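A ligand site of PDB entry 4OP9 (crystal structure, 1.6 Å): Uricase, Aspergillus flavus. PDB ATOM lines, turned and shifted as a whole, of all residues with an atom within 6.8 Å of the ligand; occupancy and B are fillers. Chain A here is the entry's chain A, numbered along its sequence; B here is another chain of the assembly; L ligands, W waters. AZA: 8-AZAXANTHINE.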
ATOM      1  N   SER A 158     -20.552 -20.901  -3.310  1.00  0.00           N
ATOM      2  CA  SER A 158     -21.407 -22.033  -3.620  1.00  0.00           C
ATOM      3  C   SER A 158     -22.140 -21.659  -4.904  1.00  0.00           C
ATOM      4  O   SER A 158     -22.610 -20.531  -5.053  1.00  0.00           O
ATOM      5  CB  SER A 158     -22.393 -22.305  -2.479  1.00  0.00           C
ATOM      6  OG  SER A 158     -23.368 -23.248  -2.882  1.00  0.00           O
ATOM      7  N   GLN A 159     -22.210 -22.611  -5.832  1.00  0.00           N
ATOM      8  CA  GLN A 159     -22.851 -22.423  -7.121  1.00  0.00           C
ATOM      9  C   GLN A 159     -23.803 -23.587  -7.376  1.00  0.00           C
ATOM     10  O   GLN A 159     -23.687 -24.681  -6.771  1.00  0.00           O
ATOM     11  CB  GLN A 159     -21.792 -22.383  -8.245  1.00  0.00           C
ATOM     12  CG  GLN A 159     -20.704 -21.344  -8.011  1.00  0.00           C
ATOM     13  CD  GLN A 159     -19.643 -21.343  -9.112  1.00  0.00           C
ATOM     14  OE1 GLN A 159     -19.843 -21.872 -10.195  1.00  0.00           O
ATOM     15  NE2 GLN A 159     -18.507 -20.727  -8.806  1.00  0.00           N
ATOM     16  N   PHE A 160     -24.728 -23.380  -8.285  1.00  0.00           N
ATOM     17  CA  PHE A 160     -25.571 -24.467  -8.758  1.00  0.00           C
ATOM     18  C   PHE A 160     -26.168 -24.114 -10.109  1.00  0.00           C
ATOM     19  O   PHE A 160     -27.122 -23.353 -10.213  1.00  0.00           O
ATOM     20  CB  PHE A 160     -26.649 -24.864  -7.722  1.00  0.00           C
ATOM     21  CG  PHE A 160     -27.313 -26.165  -8.053  1.00  0.00           C
ATOM     22  CD1 PHE A 160     -26.579 -27.338  -8.097  1.00  0.00           C
ATOM     23  CD2 PHE A 160     -28.670 -26.217  -8.396  1.00  0.00           C
ATOM     24  CE1 PHE A 160     -27.158 -28.542  -8.456  1.00  0.00           C
ATOM     25  CE2 PHE A 160     -29.260 -27.421  -8.741  1.00  0.00           C
ATOM     26  CZ  PHE A 160     -28.498 -28.581  -8.793  1.00  0.00           C
ATOM     27  N   PHE A 163     -27.941 -27.900 -14.263  1.00  0.00           N
ATOM     28  CA  PHE A 163     -28.857 -29.008 -14.003  1.00  0.00           C
ATOM     29  C   PHE A 163     -29.911 -29.195 -15.098  1.00  0.00           C
ATOM     30  O   PHE A 163     -30.098 -28.312 -15.934  1.00  0.00           O
ATOM     31  CB  PHE A 163     -29.544 -28.830 -12.631  1.00  0.00           C
ATOM     32  CG  PHE A 163     -30.136 -27.463 -12.426  1.00  0.00           C
ATOM     33  CD1 PHE A 163     -29.382 -26.433 -11.891  1.00  0.00           C
ATOM     34  CD2 PHE A 163     -31.472 -27.215 -12.784  1.00  0.00           C
ATOM     35  CE1 PHE A 163     -29.911 -25.163 -11.693  1.00  0.00           C
ATOM     36  CE2 PHE A 163     -32.019 -25.955 -12.600  1.00  0.00           C
ATOM     37  CZ  PHE A 163     -31.241 -24.935 -12.075  1.00  0.00           C
ATOM     38  N   LEU A 171     -36.388 -23.258 -11.272  1.00  0.00           N
ATOM     39  CA  LEU A 171     -35.166 -22.790 -10.586  1.00  0.00           C
ATOM     40  C   LEU A 171     -34.189 -22.088 -11.535  1.00  0.00           C
ATOM     41  O   LEU A 171     -33.842 -22.652 -12.579  1.00  0.00           O
ATOM     42  CB  LEU A 171     -34.462 -23.989  -9.906  1.00  0.00           C
ATOM     43  CG  LEU A 171     -33.201 -23.696  -9.059  1.00  0.00           C
ATOM     44  CD1 LEU A 171     -33.561 -22.882  -7.833  1.00  0.00           C
ATOM     45  CD2 LEU A 171     -32.557 -25.006  -8.645  1.00  0.00           C
ATOM     46  N   ARG A 177     -24.440 -18.385  -4.258  1.00  0.00           N
ATOM     47  CA  ARG A 177     -25.571 -18.574  -3.326  1.00  0.00           C
ATOM     48  C   ARG A 177     -25.041 -18.886  -1.941  1.00  0.00           C
ATOM     49  O   ARG A 177     -23.853 -19.174  -1.736  1.00  0.00           O
ATOM     50  CB  ARG A 177     -26.484 -19.702  -3.812  1.00  0.00           C
ATOM     51  CG  ARG A 177     -25.811 -21.061  -3.734  1.00  0.00           C
ATOM     52  CD  ARG A 177     -26.721 -22.164  -4.217  1.00  0.00           C
ATOM     53  NE  ARG A 177     -26.069 -23.473  -4.014  1.00  0.00           N
ATOM     54  CZ  ARG A 177     -26.663 -24.654  -4.146  1.00  0.00           C
ATOM     55  NH1 ARG A 177     -27.937 -24.766  -4.524  1.00  0.00           N
ATOM     56  NH2 ARG A 177     -25.960 -25.765  -3.916  1.00  0.00           N
ATOM     57  N   LEU A 179     -24.943 -21.467   1.161  1.00  0.00           N
ATOM     58  CA  LEU A 179     -25.051 -22.897   1.396  1.00  0.00           C
ATOM     59  C   LEU A 179     -25.021 -23.139   2.906  1.00  0.00           C
ATOM     60  O   LEU A 179     -24.071 -22.741   3.592  1.00  0.00           O
ATOM     61  CB  LEU A 179     -23.917 -23.667   0.698  1.00  0.00           C
ATOM     62  CG  LEU A 179     -23.952 -25.186   0.859  1.00  0.00           C
ATOM     63  CD1 LEU A 179     -25.256 -25.776   0.323  1.00  0.00           C
ATOM     64  CD2 LEU A 179     -22.758 -25.813   0.142  1.00  0.00           C
ATOM     65  N   SER A 225     -18.028 -24.713  -4.209  1.00  0.00           N
ATOM     66  CA  SER A 225     -18.912 -25.840  -4.349  1.00  0.00           C
ATOM     67  C   SER A 225     -19.768 -25.804  -5.612  1.00  0.00           C
ATOM     68  O   SER A 225     -20.480 -24.831  -5.862  1.00  0.00           O
ATOM     69  CB  SER A 225     -19.795 -25.923  -3.100  1.00  0.00           C
ATOM     70  OG  SER A 225     -20.774 -26.913  -3.274  1.00  0.00           O
ATOM     71  N   ALA A 226     -19.730 -26.886  -6.375  1.00  0.00           N
ATOM     72  CA  ALA A 226     -20.500 -26.994  -7.595  1.00  0.00           C
ATOM     73  C   ALA A 226     -21.896 -27.525  -7.301  1.00  0.00           C
ATOM     74  O   ALA A 226     -22.812 -27.419  -8.142  1.00  0.00           O
ATOM     75  CB  ALA A 226     -19.754 -27.929  -8.576  1.00  0.00           C
ATOM     76  N   SER A 227     -22.052 -28.099  -6.107  1.00  0.00           N
ATOM     77  CA  SER A 227     -23.328 -28.697  -5.660  1.00  0.00           C
ATOM     78  C   SER A 227     -23.043 -29.321  -4.304  1.00  0.00           C
ATOM     79  O   SER A 227     -21.896 -29.536  -3.945  1.00  0.00           O
ATOM     80  CB  SER A 227     -23.865 -29.796  -6.592  1.00  0.00           C
ATOM     81  OG  SER A 227     -22.987 -30.930  -6.601  1.00  0.00           O
ATOM     82  N   VAL A 228     -24.094 -29.640  -3.553  1.00  0.00           N
ATOM     83  CA  VAL A 228     -23.902 -30.357  -2.295  1.00  0.00           C
ATOM     84  C   VAL A 228     -23.265 -31.720  -2.599  1.00  0.00           C
ATOM     85  O   VAL A 228     -22.333 -32.159  -1.884  1.00  0.00           O
ATOM     86  CB  VAL A 228     -25.264 -30.487  -1.563  1.00  0.00           C
ATOM     87  CG1 VAL A 228     -25.148 -31.390  -0.345  1.00  0.00           C
ATOM     88  CG2 VAL A 228     -25.738 -29.090  -1.147  1.00  0.00           C
ATOM     89  N   GLN A 229     -23.785 -32.370  -3.646  1.00  0.00           N
ATOM     90  CA  GLN A 229     -23.296 -33.678  -4.118  1.00  0.00           C
ATOM     91  C   GLN A 229     -21.781 -33.666  -4.288  1.00  0.00           C
ATOM     92  O   GLN A 229     -21.073 -34.562  -3.771  1.00  0.00           O
ATOM     93  CB  GLN A 229     -23.957 -34.015  -5.464  1.00  0.00           C
ATOM     94  CG  GLN A 229     -25.434 -34.433  -5.372  1.00  0.00           C
ATOM     95  CD  GLN A 229     -26.415 -33.292  -5.450  1.00  0.00           C
ATOM     96  OE1 GLN A 229     -26.102 -32.142  -5.130  1.00  0.00           O
ATOM     97  NE2 GLN A 229     -27.638 -33.626  -5.859  1.00  0.00           N
ATOM     98  N   ASN A 255     -30.202 -29.389   2.452  1.00  0.00           N
ATOM     99  CA  ASN A 255     -29.859 -28.124   1.866  1.00  0.00           C
ATOM    100  C   ASN A 255     -30.855 -27.116   2.459  1.00  0.00           C
ATOM    101  O   ASN A 255     -32.006 -27.152   2.084  1.00  0.00           O
ATOM    102  CB  ASN A 255     -29.938 -28.254   0.333  1.00  0.00           C
ATOM    103  CG  ASN A 255     -29.371 -27.047  -0.391  1.00  0.00           C
ATOM    104  OD1 ASN A 255     -28.862 -26.117   0.227  1.00  0.00           O
ATOM    105  ND2 ASN A 255     -29.485 -27.058  -1.721  1.00  0.00           N
ATOM    106  N   HIS A 257     -32.423 -23.820   2.706  1.00  0.00           N
ATOM    107  CA  HIS A 257     -32.476 -22.745   1.718  1.00  0.00           C
ATOM    108  C   HIS A 257     -32.628 -21.391   2.318  1.00  0.00           C
ATOM    109  O   HIS A 257     -33.370 -21.187   3.269  1.00  0.00           O
ATOM    110  CB  HIS A 257     -33.608 -22.999   0.724  1.00  0.00           C
ATOM    111  CG  HIS A 257     -33.539 -24.353   0.078  1.00  0.00           C
ATOM    112  ND1 HIS A 257     -32.523 -24.704  -0.743  1.00  0.00           N
ATOM    113  CD2 HIS A 257     -34.386 -25.457   0.156  1.00  0.00           C
ATOM    114  CE1 HIS A 257     -32.730 -25.976  -1.184  1.00  0.00           C
ATOM    115  NE2 HIS A 257     -33.866 -26.433  -0.629  1.00  0.00           N
ATOM    116  N   GLY A 287     -33.921 -29.458   0.559  1.00  0.00           N
ATOM    117  CA  GLY A 287     -33.234 -30.536  -0.169  1.00  0.00           C
ATOM    118  C   GLY A 287     -32.622 -31.515   0.816  1.00  0.00           C
ATOM    119  O   GLY A 287     -32.313 -31.171   1.961  1.00  0.00           O
ATOM    120  N   ILE A 289     -29.696 -34.654   0.552  1.00  0.00           N
ATOM    121  CA  ILE A 289     -28.732 -35.260  -0.362  1.00  0.00           C
ATOM    122  C   ILE A 289     -27.951 -36.288   0.441  1.00  0.00           C
ATOM    123  O   ILE A 289     -27.433 -35.966   1.519  1.00  0.00           O
ATOM    124  CB  ILE A 289     -27.750 -34.192  -0.913  1.00  0.00           C
ATOM    125  CG1 ILE A 289     -28.487 -32.889  -1.329  1.00  0.00           C
ATOM    126  CG2 ILE A 289     -26.917 -34.790  -2.048  1.00  0.00           C
ATOM    127  CD1 ILE A 289     -29.514 -33.031  -2.403  1.00  0.00           C
ATOM    128  N   TYR B   9     -31.167 -38.644  -3.486  1.00  0.00           N
ATOM    129  CA  TYR B   9     -31.296 -37.226  -3.167  1.00  0.00           C
ATOM    130  C   TYR B   9     -32.730 -36.801  -3.548  1.00  0.00           C
ATOM    131  O   TYR B   9     -33.410 -37.437  -4.353  1.00  0.00           O
ATOM    132  CB  TYR B   9     -30.235 -36.382  -3.906  1.00  0.00           C
ATOM    133  CG  TYR B   9     -30.678 -36.079  -5.309  1.00  0.00           C
ATOM    134  CD1 TYR B   9     -30.709 -37.082  -6.272  1.00  0.00           C
ATOM    135  CD2 TYR B   9     -31.179 -34.833  -5.641  1.00  0.00           C
ATOM    136  CE1 TYR B   9     -31.203 -36.829  -7.545  1.00  0.00           C
ATOM    137  CE2 TYR B   9     -31.667 -34.569  -6.909  1.00  0.00           C
ATOM    138  CZ  TYR B   9     -31.686 -35.580  -7.855  1.00  0.00           C
ATOM    139  OH  TYR B   9     -32.190 -35.332  -9.105  1.00  0.00           O
ATOM    140  N   GLY B  10     -33.197 -35.707  -2.959  1.00  0.00           N
ATOM    141  CA  GLY B  10     -34.534 -35.230  -3.312  1.00  0.00           C
ATOM    142  C   GLY B  10     -34.969 -34.109  -2.398  1.00  0.00           C
ATOM    143  O   GLY B  10     -34.162 -33.341  -1.907  1.00  0.00           O
ATOM    144  N   LYS B  11     -36.276 -34.028  -2.146  1.00  0.00           N
ATOM    145  CA  LYS B  11     -36.833 -32.903  -1.363  1.00  0.00           C
ATOM    146  C   LYS B  11     -37.571 -33.494  -0.186  1.00  0.00           C
ATOM    147  O   LYS B  11     -38.321 -34.447  -0.373  1.00  0.00           O
ATOM    148  CB  LYS B  11     -37.785 -32.060  -2.201  1.00  0.00           C
ATOM    149  CG  LYS B  11     -38.006 -30.648  -1.651  1.00  0.00           C
ATOM    150  CD  LYS B  11     -36.721 -29.830  -1.680  1.00  0.00           C
ATOM    151  CE  LYS B  11     -36.875 -28.508  -2.393  1.00  0.00           C
ATOM    152  NZ  LYS B  11     -35.533 -27.883  -2.613  1.00  0.00           N
ATOM    153  N   ASN B  52     -23.695 -31.705 -13.243  1.00  0.00           N
ATOM    154  CA  ASN B  52     -25.076 -31.444 -12.829  1.00  0.00           C
ATOM    155  C   ASN B  52     -26.140 -31.837 -13.857  1.00  0.00           C
ATOM    156  O   ASN B  52     -27.335 -31.785 -13.557  1.00  0.00           O
ATOM    157  CB  ASN B  52     -25.250 -30.008 -12.330  1.00  0.00           C
ATOM    158  CG  ASN B  52     -24.503 -29.739 -11.025  1.00  0.00           C
ATOM    159  OD1 ASN B  52     -24.256 -30.667 -10.260  1.00  0.00           O
ATOM    160  ND2 ASN B  52     -24.147 -28.485 -10.768  1.00  0.00           N
ATOM    161  N   ILE B  55     -28.853 -34.160 -12.789  1.00  0.00           N
ATOM    162  CA  ILE B  55     -29.678 -33.788 -11.623  1.00  0.00           C
ATOM    163  C   ILE B  55     -31.002 -33.148 -12.011  1.00  0.00           C
ATOM    164  O   ILE B  55     -31.037 -32.078 -12.631  1.00  0.00           O
ATOM    165  CB  ILE B  55     -28.947 -32.837 -10.665  1.00  0.00           C
ATOM    166  CG1 ILE B  55     -27.687 -33.494 -10.090  1.00  0.00           C
ATOM    167  CG2 ILE B  55     -29.875 -32.405  -9.495  1.00  0.00           C
ATOM    168  CD1 ILE B  55     -26.803 -32.504  -9.342  1.00  0.00           C
ATOM    169  N   VAL B  56     -32.093 -33.820 -11.658  1.00  0.00           N
ATOM    170  CA  VAL B  56     -33.398 -33.227 -11.610  1.00  0.00           C
ATOM    171  C   VAL B  56     -33.363 -32.405 -10.320  1.00  0.00           C
ATOM    172  O   VAL B  56     -33.269 -32.992  -9.242  1.00  0.00           O
ATOM    173  CB  VAL B  56     -34.476 -34.328 -11.566  1.00  0.00           C
ATOM    174  CG1 VAL B  56     -35.894 -33.757 -11.409  1.00  0.00           C
ATOM    175  CG2 VAL B  56     -34.374 -35.188 -12.839  1.00  0.00           C
ATOM    176  N   ALA B  57     -33.440 -31.068 -10.430  1.00  0.00           N
ATOM    177  CA  ALA B  57     -33.268 -30.201  -9.252  1.00  0.00           C
ATOM    178  C   ALA B  57     -34.279 -30.552  -8.175  1.00  0.00           C
ATOM    179  O   ALA B  57     -35.411 -30.884  -8.480  1.00  0.00           O
ATOM    180  CB  ALA B  57     -33.369 -28.723  -9.637  1.00  0.00           C
ATOM    181  N   THR B  58     -33.873 -30.460  -6.910  1.00  0.00           N
ATOM    182  CA  THR B  58     -34.794 -30.762  -5.842  1.00  0.00           C
ATOM    183  C   THR B  58     -35.949 -29.774  -5.890  1.00  0.00           C
ATOM    184  O   THR B  58     -37.080 -30.150  -5.579  1.00  0.00           O
ATOM    185  CB  THR B  58     -34.130 -30.772  -4.453  1.00  0.00           C
ATOM    186  OG1 THR B  58     -33.693 -29.450  -4.123  1.00  0.00           O
ATOM    187  CG2 THR B  58     -32.943 -31.755  -4.454  1.00  0.00           C
ATOM    188  N   ASP B  59     -35.691 -28.527  -6.299  1.00  0.00           N
ATOM    189  CA  ASP B  59     -36.771 -27.560  -6.487  1.00  0.00           C
ATOM    190  C   ASP B  59     -37.813 -28.057  -7.496  1.00  0.00           C
ATOM    191  O   ASP B  59     -38.994 -27.836  -7.298  1.00  0.00           O
ATOM    192  CB  ASP B  59     -36.202 -26.228  -6.939  1.00  0.00           C
ATOM    193  CG  ASP B  59     -37.237 -25.133  -6.896  1.00  0.00           C
ATOM    194  OD1 ASP B  59     -37.518 -24.615  -5.783  1.00  0.00           O
ATOM    195  OD2 ASP B  59     -37.758 -24.786  -7.982  1.00  0.00           O
ATOM    196  N   SER B  60     -37.358 -28.695  -8.576  1.00  0.00           N
ATOM    197  CA  SER B  60     -38.276 -29.286  -9.565  1.00  0.00           C
ATOM    198  C   SER B  60     -39.060 -30.450  -9.006  1.00  0.00           C
ATOM    199  O   SER B  60     -40.219 -30.691  -9.372  1.00  0.00           O
ATOM    200  CB  SER B  60     -37.501 -29.722 -10.831  1.00  0.00           C
ATOM    201  OG  SER B  60     -36.717 -28.638 -11.261  1.00  0.00           O
HETATM  202  N1  AZA L   1     -28.073 -29.944  -5.217  1.00  0.00           N
HETATM  203  C2  AZA L   1     -27.786 -28.685  -4.831  1.00  0.00           C
HETATM  204  O2  AZA L   1     -26.679 -28.462  -4.328  1.00  0.00           O
HETATM  205  N3  AZA L   1     -28.663 -27.642  -4.911  1.00  0.00           N
HETATM  206  C4  AZA L   1     -29.871 -27.870  -5.460  1.00  0.00           C
HETATM  207  C5  AZA L   1     -30.244 -29.213  -5.917  1.00  0.00           C
HETATM  208  C6  AZA L   1     -29.244 -30.286  -5.779  1.00  0.00           C
HETATM  209  O6  AZA L   1     -29.529 -31.458  -6.127  1.00  0.00           O
HETATM  210  N7  AZA L   1     -31.495 -29.152  -6.420  1.00  0.00           N
HETATM  211  N8  AZA L   1     -31.916 -27.853  -6.267  1.00  0.00           N
HETATM  212  N9  AZA L   1     -30.917 -27.067  -5.701  1.00  0.00           N
HETATM  213  O   HOH W   1     -31.419 -29.154  -2.595  1.00  0.00           O
HETATM  214  O   HOH W   2     -31.342 -24.568  -4.780  1.00  0.00           O
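Phe 160 touches the ligand (CE2 to C4, 3.4 Å).
Leu 171 touches the ligand (CD2 to N8, 3.8 Å).
Ser 227 touches the ligand.
Tyr 9 of chain B touches the ligand.
Ile 55 of chain B touches the ligand (CG2 to O6, 3.5 Å).
Ala 57 of chain B touches the ligand (CA to N7, 3.5 Å).
Asp 59 of chain B touches the ligand (N to N8, 3.8 Å).
Hydrophobic or aromatic side chains within 4 Å of the ligand: Phe 160, Leu 171, Val 228, Tyr 9 of chain B, Ile 55 of chain B and Ala 57 of chain B.
Of the 26 residues printed, 12 come within 4 Å of the ligand.
The nearest printed residue that does not touch the ligand is Ile 289 (4.04 Å).
The backbone NH (N) of Val 228 sits at hydrogen-bond distance from an oxygen (O2) of the ligand (2.9 Å).
The side-chain hydroxyl (OG1) of Thr 58 of chain B lies within hydrogen-bond range of a nitrogen (N7) of the ligand, 3.2 Å away.
NH2 of Arg 177 lies within hydrogen-bond range of O2 of the ligand.
The side-chain amide nitrogen (ND2) of Asn 255 sits close to a nitrogen (N3) of the ligand (3.3 Å).
An oxygen (O6) of the ligand lies within hydrogen-bond range of the side-chain amide nitrogen (NE2) of Gln 229 (2.9 Å).
N7 of the ligand lies within hydrogen-bond range of N of Thr 58 of chain B (2.8 Å).
Water W2 bridges a nitrogen (N9) of the ligand (2.7 Å) and the guanidinium group of Arg 177 (3.4 Å).
Water W1 lies within hydrogen-bond range of OG1 of Thr 58 of chain B (2.8 Å) and ND2 of Asn 255 (3.0 Å).
N of Asn 255 sits at hydrogen-bond distance from O of Gly 287 (2.8 Å).
O of Ser 227 lies within hydrogen-bond range of OG of Ser 225 (2.9 Å).
The backbone NH (N) of Gln 229 lies close to the side-chain hydroxyl (OG) of Ser 227 (3.4 Å).
O of Asn 255 is in hydrogen-bond range of NE2 of His 257.
NZ of Lys 11 of chain B is in hydrogen-bond range of OG1 of Thr 58 of chain B, 2.8 Å away.
The backbone NH of Arg 177 sits at hydrogen-bond distance from the backbone carbonyl oxygen of Ser 158 (2.9 Å).
The backbone carbonyl oxygen (O) of Val 56 of chain B lies within hydrogen-bond range of the side-chain hydroxyl (OH) of Tyr 9 of chain B (2.6 Å).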
